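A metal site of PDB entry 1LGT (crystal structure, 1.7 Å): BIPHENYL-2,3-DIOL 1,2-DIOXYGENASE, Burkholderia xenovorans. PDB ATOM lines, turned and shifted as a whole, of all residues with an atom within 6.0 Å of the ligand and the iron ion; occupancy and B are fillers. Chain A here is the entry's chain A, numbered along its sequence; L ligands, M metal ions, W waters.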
ATOM      1  N   HIS A 145       1.743 -25.860  17.041  1.00  0.00           N
ATOM      2  CA  HIS A 145       1.608 -26.532  18.335  1.00  0.00           C
ATOM      3  C   HIS A 145       1.185 -25.586  19.444  1.00  0.00           C
ATOM      4  O   HIS A 145       1.118 -24.372  19.244  1.00  0.00           O
ATOM      5  CB  HIS A 145       2.925 -27.232  18.749  1.00  0.00           C
ATOM      6  CG  HIS A 145       4.036 -26.297  19.151  1.00  0.00           C
ATOM      7  ND1 HIS A 145       5.148 -26.066  18.359  1.00  0.00           N
ATOM      8  CD2 HIS A 145       4.226 -25.556  20.274  1.00  0.00           C
ATOM      9  CE1 HIS A 145       5.968 -25.241  18.987  1.00  0.00           C
ATOM     10  NE2 HIS A 145       5.431 -24.915  20.151  1.00  0.00           N
ATOM     11  N   VAL A 147       1.238 -25.405  24.052  1.00  0.00           N
ATOM     12  CA  VAL A 147       1.702 -26.016  25.278  1.00  0.00           C
ATOM     13  C   VAL A 147       0.611 -25.988  26.320  1.00  0.00           C
ATOM     14  O   VAL A 147       0.193 -24.928  26.796  1.00  0.00           O
ATOM     15  CB  VAL A 147       2.952 -25.287  25.800  1.00  0.00           C
ATOM     16  CG1 VAL A 147       3.494 -25.988  27.041  1.00  0.00           C
ATOM     17  CG2 VAL A 147       4.001 -25.233  24.707  1.00  0.00           C
ATOM     18  N   ILE A 172      12.230 -31.965  28.467  1.00  0.00           N
ATOM     19  CA  ILE A 172      13.131 -30.898  28.873  1.00  0.00           C
ATOM     20  C   ILE A 172      12.820 -30.576  30.314  1.00  0.00           C
ATOM     21  O   ILE A 172      11.702 -30.205  30.649  1.00  0.00           O
ATOM     22  CB  ILE A 172      12.940 -29.615  28.024  1.00  0.00           C
ATOM     23  CG1 ILE A 172      13.261 -29.903  26.558  1.00  0.00           C
ATOM     24  CG2 ILE A 172      13.876 -28.522  28.546  1.00  0.00           C
ATOM     25  CD1 ILE A 172      13.193 -28.686  25.665  1.00  0.00           C
ATOM     26  N   MET A 174      12.790 -28.184  32.792  1.00  0.00           N
ATOM     27  CA  MET A 174      12.825 -26.726  32.888  1.00  0.00           C
ATOM     28  C   MET A 174      13.169 -26.207  34.270  1.00  0.00           C
ATOM     29  O   MET A 174      12.458 -26.477  35.232  1.00  0.00           O
ATOM     30  CB  MET A 174      11.457 -26.161  32.512  1.00  0.00           C
ATOM     31  CG  MET A 174      10.915 -26.628  31.177  1.00  0.00           C
ATOM     32  SD  MET A 174      11.551 -25.659  29.821  1.00  0.00           S
ATOM     33  CE  MET A 174      10.535 -26.260  28.462  1.00  0.00           C
ATOM     34  N   ALA A 184       8.935 -30.831  30.962  1.00  0.00           N
ATOM     35  CA  ALA A 184       8.035 -30.440  29.897  1.00  0.00           C
ATOM     36  C   ALA A 184       8.126 -31.583  28.889  1.00  0.00           C
ATOM     37  O   ALA A 184       9.225 -31.978  28.498  1.00  0.00           O
ATOM     38  CB  ALA A 184       8.487 -29.139  29.252  1.00  0.00           C
ATOM     39  N   PHE A 186       7.274 -33.129  25.157  1.00  0.00           N
ATOM     40  CA  PHE A 186       6.966 -32.711  23.782  1.00  0.00           C
ATOM     41  C   PHE A 186       6.508 -33.938  23.007  1.00  0.00           C
ATOM     42  O   PHE A 186       7.228 -34.930  22.914  1.00  0.00           O
ATOM     43  CB  PHE A 186       8.201 -32.059  23.151  1.00  0.00           C
ATOM     44  CG  PHE A 186       8.643 -30.832  23.888  1.00  0.00           C
ATOM     45  CD1 PHE A 186       9.383 -30.934  25.073  1.00  0.00           C
ATOM     46  CD2 PHE A 186       8.251 -29.567  23.455  1.00  0.00           C
ATOM     47  CE1 PHE A 186       9.700 -29.798  25.813  1.00  0.00           C
ATOM     48  CE2 PHE A 186       8.574 -28.423  24.190  1.00  0.00           C
ATOM     49  CZ  PHE A 186       9.298 -28.541  25.376  1.00  0.00           C
ATOM     50  N   HIS A 194       6.858 -31.471  17.516  1.00  0.00           N
ATOM     51  CA  HIS A 194       5.796 -31.549  18.500  1.00  0.00           C
ATOM     52  C   HIS A 194       4.589 -30.726  18.074  1.00  0.00           C
ATOM     53  O   HIS A 194       4.725 -29.647  17.488  1.00  0.00           O
ATOM     54  CB  HIS A 194       6.249 -31.150  19.931  1.00  0.00           C
ATOM     55  CG  HIS A 194       6.819 -29.774  20.055  1.00  0.00           C
ATOM     56  ND1 HIS A 194       8.092 -29.452  19.648  1.00  0.00           N
ATOM     57  CD2 HIS A 194       6.300 -28.641  20.607  1.00  0.00           C
ATOM     58  CE1 HIS A 194       8.344 -28.190  19.944  1.00  0.00           C
ATOM     59  NE2 HIS A 194       7.275 -27.672  20.522  1.00  0.00           N
ATOM     60  N   ALA A 197       2.731 -29.923  23.757  1.00  0.00           N
ATOM     61  CA  ALA A 197       3.717 -30.019  24.826  1.00  0.00           C
ATOM     62  C   ALA A 197       2.881 -29.978  26.099  1.00  0.00           C
ATOM     63  O   ALA A 197       1.800 -29.376  26.108  1.00  0.00           O
ATOM     64  CB  ALA A 197       4.683 -28.844  24.778  1.00  0.00           C
ATOM     65  N   ALA A 199       3.203 -29.401  30.437  1.00  0.00           N
ATOM     66  CA  ALA A 199       4.045 -28.993  31.560  1.00  0.00           C
ATOM     67  C   ALA A 199       3.219 -28.425  32.696  1.00  0.00           C
ATOM     68  O   ALA A 199       2.137 -27.875  32.485  1.00  0.00           O
ATOM     69  CB  ALA A 199       5.070 -27.958  31.088  1.00  0.00           C
ATOM     70  N   PHE A 201       3.243 -25.666  34.628  1.00  0.00           N
ATOM     71  CA  PHE A 201       3.690 -24.297  34.834  1.00  0.00           C
ATOM     72  C   PHE A 201       2.688 -23.534  35.694  1.00  0.00           C
ATOM     73  O   PHE A 201       1.490 -23.791  35.638  1.00  0.00           O
ATOM     74  CB  PHE A 201       3.841 -23.542  33.513  1.00  0.00           C
ATOM     75  CG  PHE A 201       4.910 -24.091  32.602  1.00  0.00           C
ATOM     76  CD1 PHE A 201       6.122 -24.515  33.115  1.00  0.00           C
ATOM     77  CD2 PHE A 201       4.694 -24.146  31.224  1.00  0.00           C
ATOM     78  CE1 PHE A 201       7.135 -24.983  32.260  1.00  0.00           C
ATOM     79  CE2 PHE A 201       5.701 -24.607  30.373  1.00  0.00           C
ATOM     80  CZ  PHE A 201       6.918 -25.029  30.894  1.00  0.00           C
ATOM     81  N   HIS A 208       0.331 -22.053  27.681  1.00  0.00           N
ATOM     82  CA  HIS A 208       1.340 -21.022  27.864  1.00  0.00           C
ATOM     83  C   HIS A 208       1.438 -20.263  26.553  1.00  0.00           C
ATOM     84  O   HIS A 208       1.515 -19.032  26.534  1.00  0.00           O
ATOM     85  CB  HIS A 208       2.687 -21.656  28.221  1.00  0.00           C
ATOM     86  CG  HIS A 208       3.837 -20.698  28.143  1.00  0.00           C
ATOM     87  ND1 HIS A 208       4.592 -20.527  27.003  1.00  0.00           N
ATOM     88  CD2 HIS A 208       4.325 -19.815  29.052  1.00  0.00           C
ATOM     89  CE1 HIS A 208       5.493 -19.590  27.203  1.00  0.00           C
ATOM     90  NE2 HIS A 208       5.354 -19.136  28.443  1.00  0.00           N
ATOM     91  N   HIS A 209       1.438 -20.990  25.448  1.00  0.00           N
ATOM     92  CA  HIS A 209       1.509 -20.371  24.134  1.00  0.00           C
ATOM     93  C   HIS A 209       1.085 -21.325  23.027  1.00  0.00           C
ATOM     94  O   HIS A 209       0.959 -22.531  23.255  1.00  0.00           O
ATOM     95  CB  HIS A 209       2.939 -19.894  23.811  1.00  0.00           C
ATOM     96  CG  HIS A 209       3.913 -21.002  23.537  1.00  0.00           C
ATOM     97  ND1 HIS A 209       4.628 -21.626  24.539  1.00  0.00           N
ATOM     98  CD2 HIS A 209       4.339 -21.561  22.371  1.00  0.00           C
ATOM     99  CE1 HIS A 209       5.454 -22.519  24.004  1.00  0.00           C
ATOM    100  NE2 HIS A 209       5.293 -22.494  22.695  1.00  0.00           N
ATOM    101  N   MET A 211       1.987 -21.907  18.745  1.00  0.00           N
ATOM    102  CA  MET A 211       3.079 -21.578  17.848  1.00  0.00           C
ATOM    103  C   MET A 211       2.681 -21.697  16.385  1.00  0.00           C
ATOM    104  O   MET A 211       1.949 -22.601  16.006  1.00  0.00           O
ATOM    105  CB  MET A 211       4.267 -22.517  18.128  1.00  0.00           C
ATOM    106  CG  MET A 211       5.540 -22.272  17.323  1.00  0.00           C
ATOM    107  SD  MET A 211       5.569 -22.976  15.647  1.00  0.00           S
ATOM    108  CE  MET A 211       4.875 -24.541  15.899  1.00  0.00           C
ATOM    109  N   HIS A 240      15.677 -23.457  19.617  1.00  0.00           N
ATOM    110  CA  HIS A 240      15.428 -24.483  20.608  1.00  0.00           C
ATOM    111  C   HIS A 240      16.371 -25.677  20.506  1.00  0.00           C
ATOM    112  O   HIS A 240      16.855 -26.018  19.428  1.00  0.00           O
ATOM    113  CB  HIS A 240      13.982 -24.979  20.496  1.00  0.00           C
ATOM    114  CG  HIS A 240      12.974 -24.005  21.014  1.00  0.00           C
ATOM    115  ND1 HIS A 240      12.978 -23.544  22.317  1.00  0.00           N
ATOM    116  CD2 HIS A 240      11.911 -23.415  20.407  1.00  0.00           C
ATOM    117  CE1 HIS A 240      11.969 -22.712  22.487  1.00  0.00           C
ATOM    118  NE2 HIS A 240      11.298 -22.618  21.343  1.00  0.00           N
ATOM    119  N   THR A 241      16.624 -26.305  21.644  1.00  0.00           N
ATOM    120  CA  THR A 241      17.496 -27.468  21.715  1.00  0.00           C
ATOM    121  C   THR A 241      16.881 -28.739  21.138  1.00  0.00           C
ATOM    122  O   THR A 241      17.598 -29.581  20.579  1.00  0.00           O
ATOM    123  CB  THR A 241      17.855 -27.775  23.181  1.00  0.00           C
ATOM    124  OG1 THR A 241      16.644 -27.817  23.952  1.00  0.00           O
ATOM    125  CG2 THR A 241      18.789 -26.733  23.751  1.00  0.00           C
ATOM    126  N   ASN A 242      15.557 -28.884  21.251  1.00  0.00           N
ATOM    127  CA  ASN A 242      14.911 -30.100  20.781  1.00  0.00           C
ATOM    128  C   ASN A 242      14.402 -30.104  19.344  1.00  0.00           C
ATOM    129  O   ASN A 242      14.747 -31.010  18.581  1.00  0.00           O
ATOM    130  CB  ASN A 242      13.796 -30.528  21.761  1.00  0.00           C
ATOM    131  CG  ASN A 242      12.713 -29.471  21.947  1.00  0.00           C
ATOM    132  OD1 ASN A 242      12.823 -28.341  21.489  1.00  0.00           O
ATOM    133  ND2 ASN A 242      11.637 -29.856  22.638  1.00  0.00           N
ATOM    134  N   ASP A 243      13.580 -29.132  18.950  1.00  0.00           N
ATOM    135  CA  ASP A 243      13.114 -29.118  17.565  1.00  0.00           C
ATOM    136  C   ASP A 243      13.960 -28.217  16.668  1.00  0.00           C
ATOM    137  O   ASP A 243      13.741 -28.156  15.451  1.00  0.00           O
ATOM    138  CB  ASP A 243      11.632 -28.721  17.504  1.00  0.00           C
ATOM    139  CG  ASP A 243      11.389 -27.257  17.783  1.00  0.00           C
ATOM    140  OD1 ASP A 243      12.302 -26.573  18.269  1.00  0.00           O
ATOM    141  OD2 ASP A 243      10.255 -26.806  17.517  1.00  0.00           O
ATOM    142  N   MET A 245      14.013 -25.103  16.285  1.00  0.00           N
ATOM    143  CA  MET A 245      13.290 -24.011  15.655  1.00  0.00           C
ATOM    144  C   MET A 245      13.874 -22.683  16.095  1.00  0.00           C
ATOM    145  O   MET A 245      14.233 -22.507  17.269  1.00  0.00           O
ATOM    146  CB  MET A 245      11.810 -24.055  16.033  1.00  0.00           C
ATOM    147  CG  MET A 245      11.020 -22.887  15.482  1.00  0.00           C
ATOM    148  SD  MET A 245       9.284 -22.986  15.894  1.00  0.00           S
ATOM    149  CE  MET A 245       8.787 -24.402  14.867  1.00  0.00           C
ATOM    150  N   TYR A 249       9.107 -15.113  21.169  1.00  0.00           N
ATOM    151  CA  TYR A 249       7.794 -15.211  21.812  1.00  0.00           C
ATOM    152  C   TYR A 249       7.279 -13.800  22.051  1.00  0.00           C
ATOM    153  O   TYR A 249       8.066 -12.865  22.206  1.00  0.00           O
ATOM    154  CB  TYR A 249       7.896 -15.940  23.156  1.00  0.00           C
ATOM    155  CG  TYR A 249       8.268 -17.408  23.072  1.00  0.00           C
ATOM    156  CD1 TYR A 249       9.571 -17.789  22.799  1.00  0.00           C
ATOM    157  CD2 TYR A 249       7.315 -18.404  23.307  1.00  0.00           C
ATOM    158  CE1 TYR A 249       9.930 -19.135  22.773  1.00  0.00           C
ATOM    159  CE2 TYR A 249       7.656 -19.752  23.280  1.00  0.00           C
ATOM    160  CZ  TYR A 249       8.968 -20.102  23.019  1.00  0.00           C
ATOM    161  OH  TYR A 249       9.323 -21.423  23.027  1.00  0.00           O
ATOM    162  N   GLU A 259       4.337 -18.099  19.841  1.00  0.00           N
ATOM    163  CA  GLU A 259       5.705 -18.329  19.421  1.00  0.00           C
ATOM    164  C   GLU A 259       5.639 -18.268  17.898  1.00  0.00           C
ATOM    165  O   GLU A 259       4.708 -18.805  17.296  1.00  0.00           O
ATOM    166  CB  GLU A 259       6.187 -19.696  19.889  1.00  0.00           C
ATOM    167  CG  GLU A 259       7.599 -20.017  19.410  1.00  0.00           C
ATOM    168  CD  GLU A 259       8.105 -21.344  19.939  1.00  0.00           C
ATOM    169  OE1 GLU A 259       7.281 -22.177  20.383  1.00  0.00           O
ATOM    170  OE2 GLU A 259       9.333 -21.555  19.911  1.00  0.00           O
ATOM    171  N   PRO A 279      15.984 -25.374  27.322  1.00  0.00           N
ATOM    172  CA  PRO A 279      15.068 -25.326  26.180  1.00  0.00           C
ATOM    173  C   PRO A 279      15.659 -24.592  24.973  1.00  0.00           C
ATOM    174  O   PRO A 279      15.108 -24.661  23.869  1.00  0.00           O
ATOM    175  CB  PRO A 279      13.858 -24.608  26.749  1.00  0.00           C
ATOM    176  CG  PRO A 279      14.507 -23.577  27.632  1.00  0.00           C
ATOM    177  CD  PRO A 279      15.585 -24.401  28.350  1.00  0.00           C
ATOM    178  N   SER A 280      16.763 -23.879  25.171  1.00  0.00           N
ATOM    179  CA  SER A 280      17.353 -23.108  24.079  1.00  0.00           C
ATOM    180  C   SER A 280      18.865 -23.277  23.904  1.00  0.00           C
ATOM    181  O   SER A 280      19.625 -23.228  24.875  1.00  0.00           O
ATOM    182  CB  SER A 280      17.024 -21.629  24.266  1.00  0.00           C
ATOM    183  OG  SER A 280      15.622 -21.434  24.350  1.00  0.00           O
HETATM  184  C1  LIG L   1       9.832 -24.590  24.556  1.00  0.00           C
HETATM  185  C2  LIG L   1       9.061 -24.475  23.377  1.00  0.00           C
HETATM  186  O1  LIG L   1       7.972 -23.648  23.309  1.00  0.00           O
HETATM  187  C3  LIG L   1       9.389 -25.215  22.216  1.00  0.00           C
HETATM  188  O2  LIG L   1       8.603 -25.075  21.078  1.00  0.00           O
HETATM  189  C4  LIG L   1      10.497 -26.094  22.208  1.00  0.00           C
HETATM  190  C5  LIG L   1      11.279 -26.214  23.393  1.00  0.00           C
HETATM  191  C6  LIG L   1      10.945 -25.467  24.556  1.00  0.00           C
HETATM  192  C7  LIG L   1       9.463 -23.801  25.783  1.00  0.00           C
HETATM  193  C8  LIG L   1       8.300 -24.098  26.549  1.00  0.00           C
HETATM  194  C9  LIG L   1       7.964 -23.332  27.698  1.00  0.00           C
HETATM  195  C10 LIG L   1       8.795 -22.258  28.100  1.00  0.00           C
HETATM  196  C11 LIG L   1       9.957 -21.953  27.344  1.00  0.00           C
HETATM  197  C12 LIG L   1      10.275 -22.721  26.195  1.00  0.00           C
HETATM  198 CL1  LIG L   1       7.183 -25.396  26.175  1.00  0.00          CL
HETATM  199 FE    FE M   1       6.820 -23.766  21.591  1.00  0.00          FE
HETATM  200  O   HOH W   1       6.122 -25.779  22.797  1.00  0.00           O
HETATM  201  O   HOH W   2       9.190 -24.431  18.300  1.00  0.00           O
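Residues that only touch the ligand: Val 147 (3.5 Å), Ile 172 (3.9 Å), Met 174 (3.7 Å), Phe 186 (3.6 Å), Phe 201 (3.7 Å), His 240 (3.3 Å), Asn 242 (3.2 Å) and Pro 279 (3.7 Å). Hydrophobic or aromatic side chains that line the ligand: His 145, Val 147, Ile 172, Met 174, Phe 186, His 194, Phe 201, His 209, His 240, Tyr 249 and Pro 279. Of the 22 residues printed, 13 come within 4 Å of the ligand. The nearest printed residue that does not touch the ligand is Asp 243 (4.3 Å).
Merely in contact with the iron ion: Tyr 249 (3.7 Å). Four residues have an atom within 4 Å of the iron ion: His 145, His 209, Tyr 249 and Glu 259. The nearest printed residue that does not touch the iron ion is His 194 (4.1 Å).
The side-chain hydroxyl (OH) of Tyr 249 sits close to an oxygen (O1) of the ligand (2.6 Å). O2 of the ligand sits close to NE2 of His 194.
OE1 of Glu 259 binds the iron ion, at 2.0 Å. O1 of the ligand binds the iron ion, 2.1 Å away. The iron ion is bound by O2 of the ligand, at 2.3 Å. The iron ion is bound by NE2 of His 209. The iron ion is bound by NE2 of His 145, at 2.3 Å. Water W1 is bound to the iron ion, 2.4 Å away. The iron ion has six donor atoms within binding distance.
OE2 of Glu 259 sits at hydrogen-bond distance from OH of Tyr 249. OE2 of Glu 259 is in hydrogen-bond range of NE2 of His 240 (2.7 Å). ND1 of His 208 lies within hydrogen-bond range of ND1 of His 209 (2.7 Å). The backbone NH of Met 211 lies within hydrogen-bond range of the backbone carbonyl oxygen of His 145, 2.7 Å away. A ring nitrogen (NE2) of His 240 sits at hydrogen-bond distance from the side-chain hydroxyl of Tyr 249 (2.9 Å). O of Met 245 lies within hydrogen-bond range of N of His 240 (2.9 Å). O of Val 147 sits at hydrogen-bond distance from N of His 208 (3.0 Å). The backbone carbonyl oxygen (O) of Ile 172 sits at hydrogen-bond distance from the backbone NH (N) of Ala 184.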
